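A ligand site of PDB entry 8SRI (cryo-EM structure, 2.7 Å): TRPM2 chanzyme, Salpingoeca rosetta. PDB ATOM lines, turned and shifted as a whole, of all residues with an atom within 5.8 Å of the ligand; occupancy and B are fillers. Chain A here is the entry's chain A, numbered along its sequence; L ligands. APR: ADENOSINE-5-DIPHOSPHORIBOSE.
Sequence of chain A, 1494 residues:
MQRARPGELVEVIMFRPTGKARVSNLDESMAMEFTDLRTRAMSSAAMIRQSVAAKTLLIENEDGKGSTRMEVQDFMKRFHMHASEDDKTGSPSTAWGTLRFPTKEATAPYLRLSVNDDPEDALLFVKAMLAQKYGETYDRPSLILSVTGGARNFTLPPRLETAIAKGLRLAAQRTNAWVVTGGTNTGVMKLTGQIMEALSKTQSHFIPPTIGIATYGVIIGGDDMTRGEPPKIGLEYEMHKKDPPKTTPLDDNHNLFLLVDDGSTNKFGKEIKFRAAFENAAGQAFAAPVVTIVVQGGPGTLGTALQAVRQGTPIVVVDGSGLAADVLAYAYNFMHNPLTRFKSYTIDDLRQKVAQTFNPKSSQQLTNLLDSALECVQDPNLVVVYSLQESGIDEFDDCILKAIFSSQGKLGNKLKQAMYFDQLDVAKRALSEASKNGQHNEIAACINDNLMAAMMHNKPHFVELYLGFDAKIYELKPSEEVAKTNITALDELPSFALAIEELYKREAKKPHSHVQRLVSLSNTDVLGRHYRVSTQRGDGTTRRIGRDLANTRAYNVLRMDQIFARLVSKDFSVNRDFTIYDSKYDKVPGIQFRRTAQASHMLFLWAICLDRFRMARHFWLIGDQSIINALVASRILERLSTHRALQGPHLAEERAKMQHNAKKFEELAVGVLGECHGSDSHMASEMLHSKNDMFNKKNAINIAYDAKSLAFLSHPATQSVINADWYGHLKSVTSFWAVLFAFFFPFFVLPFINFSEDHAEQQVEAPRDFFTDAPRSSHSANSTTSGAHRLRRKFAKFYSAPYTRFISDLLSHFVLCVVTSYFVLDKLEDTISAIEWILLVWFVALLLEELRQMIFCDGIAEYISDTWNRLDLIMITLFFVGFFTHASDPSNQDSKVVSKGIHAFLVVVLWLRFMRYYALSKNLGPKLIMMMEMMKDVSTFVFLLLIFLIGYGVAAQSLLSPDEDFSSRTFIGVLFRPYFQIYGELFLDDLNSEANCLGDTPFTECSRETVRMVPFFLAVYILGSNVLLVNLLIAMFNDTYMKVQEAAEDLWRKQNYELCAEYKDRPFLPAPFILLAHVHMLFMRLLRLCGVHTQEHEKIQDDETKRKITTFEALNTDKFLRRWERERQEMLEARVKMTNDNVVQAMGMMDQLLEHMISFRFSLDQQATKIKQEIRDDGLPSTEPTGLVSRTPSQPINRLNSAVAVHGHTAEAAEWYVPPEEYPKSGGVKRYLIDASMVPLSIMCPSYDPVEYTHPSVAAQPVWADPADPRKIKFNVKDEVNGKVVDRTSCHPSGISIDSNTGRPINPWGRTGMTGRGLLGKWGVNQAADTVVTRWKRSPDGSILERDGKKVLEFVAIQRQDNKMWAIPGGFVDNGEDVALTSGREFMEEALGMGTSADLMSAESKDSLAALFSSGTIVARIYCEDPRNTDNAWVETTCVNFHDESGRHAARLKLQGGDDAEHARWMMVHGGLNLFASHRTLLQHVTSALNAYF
The side-chain hydroxyl (OG1) of Thr 148 lies within hydrogen-bond range of an oxygen (O1D) of the ligand. The guanidinium group of Arg 275 lies within hydrogen-bond range of an oxygen (O2D) of the ligand (2.9 Å). A nitrogen (N1) of the ligand sits at hydrogen-bond distance from the side-chain hydroxyl of Thr 184 (2.9 Å). N of Gly 300 lies within hydrogen-bond range of O2B of the ligand, at 3.0 Å. O1D of the ligand is in hydrogen-bond range of N of Gly 149, 3.1 Å away. An oxygen (O1D) of the ligand sits close to the backbone carbonyl oxygen (O) of Gly 149, 3.3 Å away. N of Ala 151 is in hydrogen-bond range of O1A of the ligand, 3.1 Å away. O2D of the ligand lies within hydrogen-bond range of OE2 of Glu 271 (3.1 Å). The backbone NH of Gly 298 sits close to an oxygen (O2B) of the ligand (3.3 Å). N of Thr 301 is in hydrogen-bond range of O2B of the ligand (3.2 Å). The side-chain hydroxyl (OG1) of Thr 301 lies close to an oxygen (O2B) of the ligand (3.5 Å).
The guanidinium group (NH2) of Arg 275 lies within hydrogen-bond range of the backbone carbonyl oxygen (O) of Val 147, 3.3 Å away. The side-chain hydroxyl (OG1) of Thr 186 sits at hydrogen-bond distance from the side-chain hydroxyl (OG1) of Thr 184 (3.2 Å). O of Gly 300 sits at hydrogen-bond distance from OG1 of Thr 304, at 2.7 Å. O of Gly 149 is in hydrogen-bond range of OG1 of Thr 301 (3.4 Å).
Merely in contact with the ligand: Gly 150 (3.3 Å), Phe 268 (3.4 Å), Arg 152 (3.5 Å), Pro 299 (3.5 Å), Thr 186 (3.6 Å), Asn 153 (3.7 Å) and Met 189 (3.9 Å). Hydrophobic or aromatic side chains that line the ligand: Ala 151, Met 189 and Phe 268. The nearest printed residue that does not touch the ligand is Thr 248 (4.03 Å).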
ATOM      1  N   VAL A 147     -13.539  23.818  16.127  1.00  0.00           N
ATOM      2  CA  VAL A 147     -12.791  23.297  17.269  1.00  0.00           C
ATOM      3  C   VAL A 147     -11.526  22.635  16.730  1.00  0.00           C
ATOM      4  O   VAL A 147     -11.602  21.636  15.996  1.00  0.00           O
ATOM      5  CB  VAL A 147     -13.626  22.317  18.115  1.00  0.00           C
ATOM      6  CG1 VAL A 147     -12.896  22.015  19.406  1.00  0.00           C
ATOM      7  CG2 VAL A 147     -14.945  22.961  18.469  1.00  0.00           C
ATOM      8  N   THR A 148     -10.369  23.180  17.082  1.00  0.00           N
ATOM      9  CA  THR A 148      -9.081  22.644  16.687  1.00  0.00           C
ATOM     10  C   THR A 148      -8.173  22.421  17.896  1.00  0.00           C
ATOM     11  O   THR A 148      -8.424  22.949  18.987  1.00  0.00           O
ATOM     12  CB  THR A 148      -8.378  23.554  15.659  1.00  0.00           C
ATOM     13  OG1 THR A 148      -7.163  22.938  15.208  1.00  0.00           O
ATOM     14  CG2 THR A 148      -8.062  24.924  16.253  1.00  0.00           C
ATOM     15  N   GLY A 149      -7.140  21.623  17.712  1.00  0.00           N
ATOM     16  CA  GLY A 149      -6.163  21.403  18.754  1.00  0.00           C
ATOM     17  C   GLY A 149      -5.427  20.069  18.619  1.00  0.00           C
ATOM     18  O   GLY A 149      -5.199  19.595  17.499  1.00  0.00           O
ATOM     19  N   GLY A 150      -5.028  19.541  19.777  1.00  0.00           N
ATOM     20  CA  GLY A 150      -4.165  18.364  19.824  1.00  0.00           C
ATOM     21  C   GLY A 150      -4.826  17.075  19.384  1.00  0.00           C
ATOM     22  O   GLY A 150      -5.891  16.693  19.908  1.00  0.00           O
ATOM     23  N   ALA A 151      -4.212  16.389  18.426  1.00  0.00           N
ATOM     24  CA  ALA A 151      -4.702  15.067  18.067  1.00  0.00           C
ATOM     25  C   ALA A 151      -4.294  13.980  19.055  1.00  0.00           C
ATOM     26  O   ALA A 151      -5.143  13.240  19.544  1.00  0.00           O
ATOM     27  CB  ALA A 151      -4.219  14.708  16.667  1.00  0.00           C
ATOM     28  N   ARG A 152      -3.040  13.975  19.506  1.00  0.00           N
ATOM     29  CA  ARG A 152      -2.563  12.935  20.418  1.00  0.00           C
ATOM     30  C   ARG A 152      -2.169  13.429  21.794  1.00  0.00           C
ATOM     31  O   ARG A 152      -2.533  12.811  22.797  1.00  0.00           O
ATOM     32  CB  ARG A 152      -1.382  12.195  19.795  1.00  0.00           C
ATOM     33  N   ASN A 153      -1.420  14.546  21.880  1.00  0.00           N
ATOM     34  CA  ASN A 153      -0.896  15.202  23.082  1.00  0.00           C
ATOM     35  C   ASN A 153      -1.959  15.841  24.015  1.00  0.00           C
ATOM     36  O   ASN A 153      -1.594  16.363  25.071  1.00  0.00           O
ATOM     37  CB  ASN A 153       0.120  16.276  22.662  1.00  0.00           C
ATOM     38  CG  ASN A 153       1.268  16.443  23.657  1.00  0.00           C
ATOM     39  OD1 ASN A 153       1.312  15.767  24.689  1.00  0.00           O
ATOM     40  ND2 ASN A 153       2.186  17.348  23.363  1.00  0.00           N
ATOM     41  N   PHE A 154      -3.253  15.806  23.662  1.00  0.00           N
ATOM     42  CA  PHE A 154      -4.364  16.321  24.450  1.00  0.00           C
ATOM     43  C   PHE A 154      -4.555  15.417  25.668  1.00  0.00           C
ATOM     44  O   PHE A 154      -5.066  14.298  25.565  1.00  0.00           O
ATOM     45  CB  PHE A 154      -5.588  16.391  23.531  1.00  0.00           C
ATOM     46  CG  PHE A 154      -6.833  16.944  24.180  1.00  0.00           C
ATOM     47  CD1 PHE A 154      -7.032  18.329  24.199  1.00  0.00           C
ATOM     48  CD2 PHE A 154      -7.873  16.093  24.602  1.00  0.00           C
ATOM     49  CE1 PHE A 154      -8.196  18.870  24.762  1.00  0.00           C
ATOM     50  CE2 PHE A 154      -9.048  16.615  25.178  1.00  0.00           C
ATOM     51  CZ  PHE A 154      -9.202  18.015  25.245  1.00  0.00           C
ATOM     52  N   GLY A 182     -11.627  18.264  13.149  1.00  0.00           N
ATOM     53  CA  GLY A 182     -10.894  17.340  12.314  1.00  0.00           C
ATOM     54  C   GLY A 182     -11.747  16.104  12.062  1.00  0.00           C
ATOM     55  O   GLY A 182     -12.618  15.751  12.858  1.00  0.00           O
ATOM     56  N   THR A 184     -10.541  13.021  12.066  1.00  0.00           N
ATOM     57  CA  THR A 184      -9.996  11.818  12.676  1.00  0.00           C
ATOM     58  C   THR A 184     -10.547  11.504  14.063  1.00  0.00           C
ATOM     59  O   THR A 184     -11.116  12.350  14.762  1.00  0.00           O
ATOM     60  CB  THR A 184      -8.485  11.954  12.750  1.00  0.00           C
ATOM     61  OG1 THR A 184      -8.148  12.932  13.747  1.00  0.00           O
ATOM     62  CG2 THR A 184      -7.920  12.439  11.407  1.00  0.00           C
ATOM     63  N   THR A 186      -9.387  10.955  17.101  1.00  0.00           N
ATOM     64  CA  THR A 186      -8.427  11.184  18.176  1.00  0.00           C
ATOM     65  C   THR A 186      -8.652  12.540  18.827  1.00  0.00           C
ATOM     66  O   THR A 186      -9.023  13.505  18.156  1.00  0.00           O
ATOM     67  CB  THR A 186      -6.972  11.132  17.649  1.00  0.00           C
ATOM     68  OG1 THR A 186      -6.842  11.900  16.440  1.00  0.00           O
ATOM     69  CG2 THR A 186      -6.333   9.715  17.520  1.00  0.00           C
ATOM     70  N   VAL A 188      -9.311  15.984  20.913  1.00  0.00           N
ATOM     71  CA  VAL A 188     -10.323  17.018  21.113  1.00  0.00           C
ATOM     72  C   VAL A 188     -11.446  16.930  20.063  1.00  0.00           C
ATOM     73  O   VAL A 188     -12.601  17.287  20.365  1.00  0.00           O
ATOM     74  CB  VAL A 188      -9.637  18.406  21.252  1.00  0.00           C
ATOM     75  CG1 VAL A 188      -9.030  18.975  19.945  1.00  0.00           C
ATOM     76  CG2 VAL A 188     -10.544  19.444  21.940  1.00  0.00           C
ATOM     77  N   MET A 189     -11.117  16.479  18.831  1.00  0.00           N
ATOM     78  CA  MET A 189     -12.078  16.250  17.757  1.00  0.00           C
ATOM     79  C   MET A 189     -13.053  15.120  18.113  1.00  0.00           C
ATOM     80  O   MET A 189     -14.260  15.230  17.882  1.00  0.00           O
ATOM     81  CB  MET A 189     -11.338  15.932  16.455  1.00  0.00           C
ATOM     82  CG  MET A 189     -10.322  16.985  16.075  1.00  0.00           C
ATOM     83  SD  MET A 189      -8.736  16.769  16.903  1.00  0.00           S
ATOM     84  CE  MET A 189      -7.887  15.709  15.739  1.00  0.00           C
ATOM     85  N   ILE A 213     -12.960  17.854   8.428  1.00  0.00           N
ATOM     86  CA  ILE A 213     -12.075  18.080   7.289  1.00  0.00           C
ATOM     87  C   ILE A 213     -10.691  17.518   7.619  1.00  0.00           C
ATOM     88  O   ILE A 213     -10.014  18.009   8.530  1.00  0.00           O
ATOM     89  CB  ILE A 213     -11.998  19.569   6.931  1.00  0.00           C
ATOM     90  CG1 ILE A 213     -13.405  20.121   6.695  1.00  0.00           C
ATOM     91  CG2 ILE A 213     -11.153  19.744   5.673  1.00  0.00           C
ATOM     92  CD1 ILE A 213     -13.474  21.588   6.284  1.00  0.00           C
ATOM     93  N   THR A 248      -4.389   6.090  10.972  1.00  0.00           N
ATOM     94  CA  THR A 248      -5.304   7.053  11.601  1.00  0.00           C
ATOM     95  C   THR A 248      -6.748   6.857  11.128  1.00  0.00           C
ATOM     96  O   THR A 248      -7.040   7.100   9.952  1.00  0.00           O
ATOM     97  CB  THR A 248      -4.821   8.470  11.316  1.00  0.00           C
ATOM     98  OG1 THR A 248      -3.497   8.630  11.832  1.00  0.00           O
ATOM     99  CG2 THR A 248      -5.687   9.434  12.055  1.00  0.00           C
ATOM    100  N   PHE A 268       0.697  15.119   7.247  1.00  0.00           N
ATOM    101  CA  PHE A 268      -0.396  15.868   7.836  1.00  0.00           C
ATOM    102  C   PHE A 268      -0.291  17.361   7.501  1.00  0.00           C
ATOM    103  O   PHE A 268       0.724  17.855   7.019  1.00  0.00           O
ATOM    104  CB  PHE A 268      -0.482  15.698   9.361  1.00  0.00           C
ATOM    105  CG  PHE A 268      -0.840  14.294   9.826  1.00  0.00           C
ATOM    106  CD1 PHE A 268       0.142  13.294   9.964  1.00  0.00           C
ATOM    107  CD2 PHE A 268      -2.194  13.956  10.003  1.00  0.00           C
ATOM    108  CE1 PHE A 268      -0.210  11.992  10.383  1.00  0.00           C
ATOM    109  CE2 PHE A 268      -2.562  12.644  10.395  1.00  0.00           C
ATOM    110  CZ  PHE A 268      -1.560  11.678  10.604  1.00  0.00           C
ATOM    111  N   GLY A 269      -1.380  18.080   7.784  1.00  0.00           N
ATOM    112  CA  GLY A 269      -1.459  19.524   7.622  1.00  0.00           C
ATOM    113  C   GLY A 269      -1.688  20.105   6.252  1.00  0.00           C
ATOM    114  O   GLY A 269      -1.534  21.321   6.084  1.00  0.00           O
ATOM    115  N   GLU A 271      -4.572  20.299   4.665  1.00  0.00           N
ATOM    116  CA  GLU A 271      -5.950  20.771   4.571  1.00  0.00           C
ATOM    117  C   GLU A 271      -6.273  22.049   5.338  1.00  0.00           C
ATOM    118  O   GLU A 271      -7.410  22.495   5.234  1.00  0.00           O
ATOM    119  CB  GLU A 271      -6.868  19.617   5.064  1.00  0.00           C
ATOM    120  CG  GLU A 271      -6.736  19.202   6.586  1.00  0.00           C
ATOM    121  CD  GLU A 271      -7.571  19.912   7.675  1.00  0.00           C
ATOM    122  OE1 GLU A 271      -8.416  20.768   7.403  1.00  0.00           O
ATOM    123  OE2 GLU A 271      -7.348  19.575   8.857  1.00  0.00           O
ATOM    124  N   ILE A 272      -5.262  22.672   5.982  1.00  0.00           N
ATOM    125  CA  ILE A 272      -5.405  23.817   6.891  1.00  0.00           C
ATOM    126  C   ILE A 272      -5.931  25.092   6.195  1.00  0.00           C
ATOM    127  O   ILE A 272      -6.906  25.707   6.671  1.00  0.00           O
ATOM    128  CB  ILE A 272      -4.035  24.066   7.560  1.00  0.00           C
ATOM    129  CG1 ILE A 272      -3.625  22.859   8.416  1.00  0.00           C
ATOM    130  CG2 ILE A 272      -3.999  25.333   8.348  1.00  0.00           C
ATOM    131  CD1 ILE A 272      -2.214  22.974   9.023  1.00  0.00           C
ATOM    132  N   ARG A 275      -9.500  24.613   4.824  1.00  0.00           N
ATOM    133  CA  ARG A 275     -10.432  24.633   5.964  1.00  0.00           C
ATOM    134  C   ARG A 275     -10.764  26.059   6.395  1.00  0.00           C
ATOM    135  O   ARG A 275     -11.935  26.374   6.624  1.00  0.00           O
ATOM    136  CB  ARG A 275      -9.833  23.838   7.135  1.00  0.00           C
ATOM    137  CG  ARG A 275     -10.717  23.722   8.361  1.00  0.00           C
ATOM    138  CD  ARG A 275     -10.032  22.952   9.479  1.00  0.00           C
ATOM    139  NE  ARG A 275     -10.663  23.181  10.772  1.00  0.00           N
ATOM    140  CZ  ARG A 275     -10.406  22.493  11.871  1.00  0.00           C
ATOM    141  NH1 ARG A 275      -9.513  21.514  11.874  1.00  0.00           N
ATOM    142  NH2 ARG A 275     -11.045  22.786  12.991  1.00  0.00           N
ATOM    143  N   GLY A 297      -3.132  21.759  21.474  1.00  0.00           N
ATOM    144  CA  GLY A 297      -2.637  21.975  20.130  1.00  0.00           C
ATOM    145  C   GLY A 297      -1.134  21.790  19.937  1.00  0.00           C
ATOM    146  O   GLY A 297      -0.334  21.871  20.874  1.00  0.00           O
ATOM    147  N   GLY A 298      -0.782  21.415  18.704  1.00  0.00           N
ATOM    148  CA  GLY A 298       0.582  21.250  18.265  1.00  0.00           C
ATOM    149  C   GLY A 298       0.998  22.381  17.318  1.00  0.00           C
ATOM    150  O   GLY A 298       0.444  23.490  17.402  1.00  0.00           O
ATOM    151  N   PRO A 299       2.071  22.162  16.522  1.00  0.00           N
ATOM    152  CA  PRO A 299       2.514  23.166  15.508  1.00  0.00           C
ATOM    153  C   PRO A 299       1.496  23.514  14.420  1.00  0.00           C
ATOM    154  O   PRO A 299       1.467  24.657  13.916  1.00  0.00           O
ATOM    155  CB  PRO A 299       3.767  22.528  14.900  1.00  0.00           C
ATOM    156  CG  PRO A 299       4.251  21.565  15.905  1.00  0.00           C
ATOM    157  CD  PRO A 299       3.031  21.039  16.592  1.00  0.00           C
ATOM    158  N   GLY A 300       0.685  22.526  13.994  1.00  0.00           N
ATOM    159  CA  GLY A 300      -0.326  22.791  12.981  1.00  0.00           C
ATOM    160  C   GLY A 300      -1.497  23.597  13.489  1.00  0.00           C
ATOM    161  O   GLY A 300      -2.195  24.228  12.684  1.00  0.00           O
ATOM    162  N   THR A 301      -1.766  23.542  14.805  1.00  0.00           N
ATOM    163  CA  THR A 301      -2.792  24.374  15.432  1.00  0.00           C
ATOM    164  C   THR A 301      -2.374  25.857  15.394  1.00  0.00           C
ATOM    165  O   THR A 301      -3.231  26.745  15.195  1.00  0.00           O
ATOM    166  CB  THR A 301      -3.014  23.826  16.850  1.00  0.00           C
ATOM    167  OG1 THR A 301      -3.569  22.503  16.743  1.00  0.00           O
ATOM    168  CG2 THR A 301      -4.003  24.613  17.662  1.00  0.00           C
ATOM    169  N   LEU A 302      -1.059  26.104  15.556  1.00  0.00           N
ATOM    170  CA  LEU A 302      -0.430  27.432  15.409  1.00  0.00           C
ATOM    171  C   LEU A 302      -0.576  27.940  13.978  1.00  0.00           C
ATOM    172  O   LEU A 302      -0.865  29.129  13.763  1.00  0.00           O
ATOM    173  CB  LEU A 302       1.048  27.383  15.811  1.00  0.00           C
ATOM    174  CG  LEU A 302       1.709  28.667  16.316  1.00  0.00           C
ATOM    175  CD1 LEU A 302       1.029  29.150  17.579  1.00  0.00           C
ATOM    176  CD2 LEU A 302       3.203  28.497  16.526  1.00  0.00           C
ATOM    177  N   THR A 304      -2.916  26.849  11.861  1.00  0.00           N
ATOM    178  CA  THR A 304      -4.373  27.001  11.731  1.00  0.00           C
ATOM    179  C   THR A 304      -4.834  28.367  12.248  1.00  0.00           C
ATOM    180  O   THR A 304      -5.650  29.043  11.602  1.00  0.00           O
ATOM    181  CB  THR A 304      -5.059  25.829  12.477  1.00  0.00           C
ATOM    182  OG1 THR A 304      -4.721  24.596  11.817  1.00  0.00           O
ATOM    183  CG2 THR A 304      -6.586  25.941  12.532  1.00  0.00           C
HETATM  184  N1  APR L   1      -5.459  13.983  13.148  1.00  0.00           N
HETATM  185  C2  APR L   1      -4.736  12.989  13.689  1.00  0.00           C
HETATM  186  N3  APR L   1      -3.402  13.054  13.858  1.00  0.00           N
HETATM  187  C4  APR L   1      -2.728  14.149  13.485  1.00  0.00           C
HETATM  188  C5  APR L   1      -3.454  15.278  12.884  1.00  0.00           C
HETATM  189  C6  APR L   1      -4.905  15.130  12.731  1.00  0.00           C
HETATM  190  N6  APR L   1      -5.653  16.118  12.177  1.00  0.00           N
HETATM  191  N7  APR L   1      -2.537  16.222  12.607  1.00  0.00           N
HETATM  192  C8  APR L   1      -1.330  15.739  13.003  1.00  0.00           C
HETATM  193  N9  APR L   1      -1.455  14.512  13.515  1.00  0.00           N
HETATM  194  C1' APR L   1      -0.350  13.688  14.055  1.00  0.00           C
HETATM  195  C2' APR L   1       0.908  14.533  14.033  1.00  0.00           C
HETATM  196  O2' APR L   1       1.971  13.781  13.455  1.00  0.00           O
HETATM  197  C3' APR L   1       1.222  14.826  15.473  1.00  0.00           C
HETATM  198  O3' APR L   1       2.566  14.459  15.753  1.00  0.00           O
HETATM  199  O4' APR L   1      -0.641  13.362  15.406  1.00  0.00           O
HETATM  200  C4' APR L   1       0.274  13.981  16.312  1.00  0.00           C
HETATM  201  C5' APR L   1      -0.470  14.819  17.337  1.00  0.00           C
HETATM  202  O5' APR L   1      -0.746  16.127  16.849  1.00  0.00           O
HETATM  203  PA  APR L   1      -0.555  17.382  17.834  1.00  0.00           P
HETATM  204  O1A APR L   1      -1.248  17.027  19.122  1.00  0.00           O
HETATM  205  O2A APR L   1       0.898  17.743  17.847  1.00  0.00           O
HETATM  206  O3A APR L   1      -1.371  18.563  17.111  1.00  0.00           O
HETATM  207  PB  APR L   1      -0.974  19.063  15.631  1.00  0.00           P
HETATM  208  O1B APR L   1       0.179  18.269  15.089  1.00  0.00           O
HETATM  209  O2B APR L   1      -0.939  20.558  15.570  1.00  0.00           O
HETATM  210  O5D APR L   1      -2.311  18.690  14.849  1.00  0.00           O
HETATM  211  C5D APR L   1      -3.298  19.696  14.810  1.00  0.00           C
HETATM  212  O4D APR L   1      -5.511  18.930  14.413  1.00  0.00           O
HETATM  213  O1D APR L   1      -7.349  20.177  15.032  1.00  0.00           O
HETATM  214  C1D APR L   1      -6.635  19.635  13.922  1.00  0.00           C
HETATM  215  O2D APR L   1      -6.700  20.646  11.725  1.00  0.00           O
HETATM  216  C2D APR L   1      -6.133  20.751  13.036  1.00  0.00           C
HETATM  217  O3D APR L   1      -4.295  20.316  11.566  1.00  0.00           O
HETATM  218  C3D APR L   1      -4.641  20.574  12.924  1.00  0.00           C
HETATM  219  C4D APR L   1      -4.317  19.361  13.758  1.00  0.00           C
